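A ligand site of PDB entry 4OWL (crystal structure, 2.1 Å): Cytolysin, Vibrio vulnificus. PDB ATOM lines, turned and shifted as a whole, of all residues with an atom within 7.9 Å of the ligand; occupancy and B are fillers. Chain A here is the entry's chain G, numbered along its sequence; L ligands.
Merely in contact with the ligand: Trp 38 and Tyr 22. Hydrophobic or aromatic side chains that line the ligand: Trp 38 and His 41. Six residues have an atom within 4 Å of the ligand: Asp 20, Val 21, Tyr 22, Trp 38, His 41 and Asn 45.
An oxygen (O3) of the ligand lies within hydrogen-bond range of the backbone carbonyl oxygen (O) of Val 21, at 3.4 Å. The side-chain carboxylate (OD1) of Asp 20 lies within hydrogen-bond range of an oxygen (O3) of the ligand (2.8 Å). A ring nitrogen (NE2) of His 41 sits at hydrogen-bond distance from an oxygen (O2) of the ligand, at 3.0 Å. The side-chain amide nitrogen (ND2) of Asn 45 sits at hydrogen-bond distance from an oxygen (O2) of the ligand, 3.2 Å away.
O of Asn 45 sits at hydrogen-bond distance from N of Val 21 (3.0 Å). ND1 of His 41 sits close to N of Ser 43. OD1 of Asp 20 is in hydrogen-bond range of ND2 of Asn 45 (3.5 Å). The side-chain amide nitrogen (NE2) of Gln 46 sits at hydrogen-bond distance from the side-chain carboxylate (OD2) of Asp 20 (2.8 Å). OH of Tyr 22 sits at hydrogen-bond distance from O of Gly 37, 2.8 Å away. The backbone NH (N) of Asp 20 sits at hydrogen-bond distance from the backbone carbonyl oxygen (O) of Asn 36 (2.9 Å). The backbone carbonyl oxygen of Trp 38 lies within hydrogen-bond range of the backbone NH of Cys 18 (2.8 Å). The backbone NH of His 41 is in hydrogen-bond range of the side-chain amide oxygen of Gln 46 (2.8 Å).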
ATOM      1  N   CYS A  18     -17.732   3.153  28.796  1.00  0.00           N
ATOM      2  CA  CYS A  18     -16.688   2.248  28.348  1.00  0.00           C
ATOM      3  C   CYS A  18     -15.503   3.065  27.862  1.00  0.00           C
ATOM      4  O   CYS A  18     -15.686   4.123  27.266  1.00  0.00           O
ATOM      5  CB  CYS A  18     -17.187   1.328  27.248  1.00  0.00           C
ATOM      6  SG  CYS A  18     -18.328   0.037  27.832  1.00  0.00           S
ATOM      7  N   ASP A  20     -12.880   4.592  25.658  1.00  0.00           N
ATOM      8  CA  ASP A  20     -13.212   4.938  24.277  1.00  0.00           C
ATOM      9  C   ASP A  20     -12.147   5.845  23.658  1.00  0.00           C
ATOM     10  O   ASP A  20     -11.710   6.825  24.285  1.00  0.00           O
ATOM     11  CB  ASP A  20     -14.582   5.626  24.250  1.00  0.00           C
ATOM     12  CG  ASP A  20     -15.070   5.963  22.829  1.00  0.00           C
ATOM     13  OD1 ASP A  20     -14.427   6.793  22.145  1.00  0.00           O
ATOM     14  OD2 ASP A  20     -16.125   5.425  22.431  1.00  0.00           O
ATOM     15  N   VAL A  21     -11.730   5.510  22.447  1.00  0.00           N
ATOM     16  CA  VAL A  21     -10.808   6.351  21.686  1.00  0.00           C
ATOM     17  C   VAL A  21     -11.557   7.520  21.053  1.00  0.00           C
ATOM     18  O   VAL A  21     -12.397   7.313  20.178  1.00  0.00           O
ATOM     19  CB  VAL A  21     -10.095   5.553  20.583  1.00  0.00           C
ATOM     20  CG1 VAL A  21      -9.142   6.439  19.801  1.00  0.00           C
ATOM     21  CG2 VAL A  21      -9.341   4.353  21.187  1.00  0.00           C
ATOM     22  N   TYR A  22     -11.253   8.751  21.489  1.00  0.00           N
ATOM     23  CA  TYR A  22     -11.853   9.946  20.873  1.00  0.00           C
ATOM     24  C   TYR A  22     -11.235  10.223  19.507  1.00  0.00           C
ATOM     25  O   TYR A  22     -11.947  10.377  18.506  1.00  0.00           O
ATOM     26  CB  TYR A  22     -11.665  11.173  21.765  1.00  0.00           C
ATOM     27  CG  TYR A  22     -12.640  11.270  22.920  1.00  0.00           C
ATOM     28  CD1 TYR A  22     -13.343  10.160  23.363  1.00  0.00           C
ATOM     29  CD2 TYR A  22     -12.839  12.486  23.571  1.00  0.00           C
ATOM     30  CE1 TYR A  22     -14.240  10.257  24.427  1.00  0.00           C
ATOM     31  CE2 TYR A  22     -13.738  12.597  24.624  1.00  0.00           C
ATOM     32  CZ  TYR A  22     -14.433  11.473  25.059  1.00  0.00           C
ATOM     33  OH  TYR A  22     -15.316  11.565  26.106  1.00  0.00           O
ATOM     34  N   GLY A  23      -9.905  10.282  19.468  1.00  0.00           N
ATOM     35  CA  GLY A  23      -9.172  10.709  18.288  1.00  0.00           C
ATOM     36  C   GLY A  23      -8.960  12.220  18.305  1.00  0.00           C
ATOM     37  O   GLY A  23      -9.067  12.844  19.364  1.00  0.00           O
ATOM     38  N   GLY A  26     -11.846  14.361  14.858  1.00  0.00           N
ATOM     39  CA  GLY A  26     -12.616  13.371  14.112  1.00  0.00           C
ATOM     40  C   GLY A  26     -11.916  12.034  13.899  1.00  0.00           C
ATOM     41  O   GLY A  26     -12.567  10.996  13.938  1.00  0.00           O
ATOM     42  N   LYS A  28     -10.255   8.798  14.461  1.00  0.00           N
ATOM     43  CA  LYS A  28     -10.089   7.828  15.546  1.00  0.00           C
ATOM     44  C   LYS A  28      -8.864   6.927  15.378  1.00  0.00           C
ATOM     45  O   LYS A  28      -8.735   5.922  16.083  1.00  0.00           O
ATOM     46  CB  LYS A  28     -11.344   6.955  15.683  1.00  0.00           C
ATOM     47  N   SER A  34      -6.830  11.313  21.715  1.00  0.00           N
ATOM     48  CA  SER A  34      -7.242  11.245  23.117  1.00  0.00           C
ATOM     49  C   SER A  34      -8.083   9.988  23.420  1.00  0.00           C
ATOM     50  O   SER A  34      -8.780   9.440  22.560  1.00  0.00           O
ATOM     51  CB  SER A  34      -8.015  12.501  23.495  1.00  0.00           C
ATOM     52  OG  SER A  34      -8.266  12.535  24.897  1.00  0.00           O
ATOM     53  N   ASN A  36     -10.874   8.791  26.389  1.00  0.00           N
ATOM     54  CA  ASN A  36     -11.717   9.165  27.524  1.00  0.00           C
ATOM     55  C   ASN A  36     -12.918   8.220  27.594  1.00  0.00           C
ATOM     56  O   ASN A  36     -12.836   7.089  27.115  1.00  0.00           O
ATOM     57  CB  ASN A  36     -12.121  10.643  27.424  1.00  0.00           C
ATOM     58  CG  ASN A  36     -11.066  11.575  28.032  1.00  0.00           C
ATOM     59  OD1 ASN A  36     -10.820  11.543  29.249  1.00  0.00           O
ATOM     60  ND2 ASN A  36     -10.451  12.396  27.202  1.00  0.00           N
ATOM     61  N   GLY A  37     -14.011   8.659  28.226  1.00  0.00           N
ATOM     62  CA  GLY A  37     -15.176   7.798  28.433  1.00  0.00           C
ATOM     63  C   GLY A  37     -16.352   8.076  27.502  1.00  0.00           C
ATOM     64  O   GLY A  37     -16.512   9.178  26.977  1.00  0.00           O
ATOM     65  N   TRP A  38     -17.186   7.071  27.324  1.00  0.00           N
ATOM     66  CA  TRP A  38     -18.330   7.183  26.424  1.00  0.00           C
ATOM     67  C   TRP A  38     -19.316   6.043  26.638  1.00  0.00           C
ATOM     68  O   TRP A  38     -18.932   4.976  27.110  1.00  0.00           O
ATOM     69  CB  TRP A  38     -17.838   7.197  24.975  1.00  0.00           C
ATOM     70  CG  TRP A  38     -18.850   7.724  24.024  1.00  0.00           C
ATOM     71  CD1 TRP A  38     -19.783   7.002  23.351  1.00  0.00           C
ATOM     72  CD2 TRP A  38     -19.038   9.086  23.648  1.00  0.00           C
ATOM     73  NE1 TRP A  38     -20.541   7.827  22.577  1.00  0.00           N
ATOM     74  CE2 TRP A  38     -20.102   9.117  22.732  1.00  0.00           C
ATOM     75  CE3 TRP A  38     -18.412  10.288  23.989  1.00  0.00           C
ATOM     76  CZ2 TRP A  38     -20.566  10.306  22.160  1.00  0.00           C
ATOM     77  CZ3 TRP A  38     -18.868  11.464  23.409  1.00  0.00           C
ATOM     78  CH2 TRP A  38     -19.935  11.460  22.514  1.00  0.00           C
ATOM     79  N   SER A  39     -20.576   6.271  26.279  1.00  0.00           N
ATOM     80  CA  SER A  39     -21.607   5.236  26.331  1.00  0.00           C
ATOM     81  C   SER A  39     -21.149   3.991  25.565  1.00  0.00           C
ATOM     82  O   SER A  39     -20.484   4.101  24.541  1.00  0.00           O
ATOM     83  CB  SER A  39     -22.934   5.769  25.739  1.00  0.00           C
ATOM     84  N   HIS A  41     -20.949   0.968  23.146  1.00  0.00           N
ATOM     85  CA  HIS A  41     -21.524   0.527  21.874  1.00  0.00           C
ATOM     86  C   HIS A  41     -20.637  -0.523  21.196  1.00  0.00           C
ATOM     87  O   HIS A  41     -21.046  -1.108  20.189  1.00  0.00           O
ATOM     88  CB  HIS A  41     -21.783   1.730  20.949  1.00  0.00           C
ATOM     89  CG  HIS A  41     -20.605   2.631  20.734  1.00  0.00           C
ATOM     90  ND1 HIS A  41     -19.419   2.191  20.175  1.00  0.00           N
ATOM     91  CD2 HIS A  41     -20.431   3.953  20.992  1.00  0.00           C
ATOM     92  CE1 HIS A  41     -18.562   3.201  20.108  1.00  0.00           C
ATOM     93  NE2 HIS A  41     -19.149   4.272  20.590  1.00  0.00           N
ATOM     94  N   GLY A  42     -19.442  -0.769  21.723  1.00  0.00           N
ATOM     95  CA  GLY A  42     -18.612  -1.886  21.290  1.00  0.00           C
ATOM     96  C   GLY A  42     -18.101  -1.828  19.857  1.00  0.00           C
ATOM     97  O   GLY A  42     -17.788  -2.862  19.265  1.00  0.00           O
ATOM     98  N   SER A  43     -18.021  -0.624  19.306  1.00  0.00           N
ATOM     99  CA  SER A  43     -17.456  -0.396  17.986  1.00  0.00           C
ATOM    100  C   SER A  43     -15.943  -0.589  18.059  1.00  0.00           C
ATOM    101  O   SER A  43     -15.395  -0.756  19.143  1.00  0.00           O
ATOM    102  CB  SER A  43     -17.796   1.002  17.486  1.00  0.00           C
ATOM    103  OG  SER A  43     -17.378   1.182  16.139  1.00  0.00           O
ATOM    104  N   ASN A  45     -13.591   1.274  18.103  1.00  0.00           N
ATOM    105  CA  ASN A  45     -12.837   2.225  18.939  1.00  0.00           C
ATOM    106  C   ASN A  45     -13.135   2.120  20.440  1.00  0.00           C
ATOM    107  O   ASN A  45     -12.794   3.010  21.215  1.00  0.00           O
ATOM    108  CB  ASN A  45     -13.111   3.654  18.471  1.00  0.00           C
ATOM    109  CG  ASN A  45     -14.529   4.065  18.713  1.00  0.00           C
ATOM    110  OD1 ASN A  45     -15.438   3.234  18.657  1.00  0.00           O
ATOM    111  ND2 ASN A  45     -14.733   5.340  19.004  1.00  0.00           N
ATOM    112  N   GLN A  46     -13.750   1.009  20.828  1.00  0.00           N
ATOM    113  CA  GLN A  46     -14.044   0.739  22.226  1.00  0.00           C
ATOM    114  C   GLN A  46     -13.565  -0.651  22.603  1.00  0.00           C
ATOM    115  O   GLN A  46     -13.773  -1.099  23.734  1.00  0.00           O
ATOM    116  CB  GLN A  46     -15.555   0.856  22.490  1.00  0.00           C
ATOM    117  CG  GLN A  46     -16.086   2.263  22.516  1.00  0.00           C
ATOM    118  CD  GLN A  46     -17.489   2.333  23.099  1.00  0.00           C
ATOM    119  OE1 GLN A  46     -18.179   1.322  23.231  1.00  0.00           O
ATOM    120  NE2 GLN A  46     -17.913   3.547  23.456  1.00  0.00           N
HETATM  121  C1  LIG L   1     -18.296   9.743  18.009  1.00  0.00           C
HETATM  122  C2  LIG L   1     -17.917   8.291  18.301  1.00  0.00           C
HETATM  123  C3  LIG L   1     -17.854   8.032  19.815  1.00  0.00           C
HETATM  124  C4  LIG L   1     -16.852   8.999  20.501  1.00  0.00           C
HETATM  125  C5  LIG L   1     -17.134  10.442  20.041  1.00  0.00           C
HETATM  126  C6  LIG L   1     -16.043  11.449  20.409  1.00  0.00           C
HETATM  127  O1  LIG L   1     -18.866   7.399  17.759  1.00  0.00           O
HETATM  128  O2  LIG L   1     -17.439   6.682  20.129  1.00  0.00           O
HETATM  129  O3  LIG L   1     -15.485   8.624  20.253  1.00  0.00           O
HETATM  130  O4  LIG L   1     -17.310  10.576  18.595  1.00  0.00           O
HETATM  131  O5  LIG L   1     -16.593  12.515  21.165  1.00  0.00           O
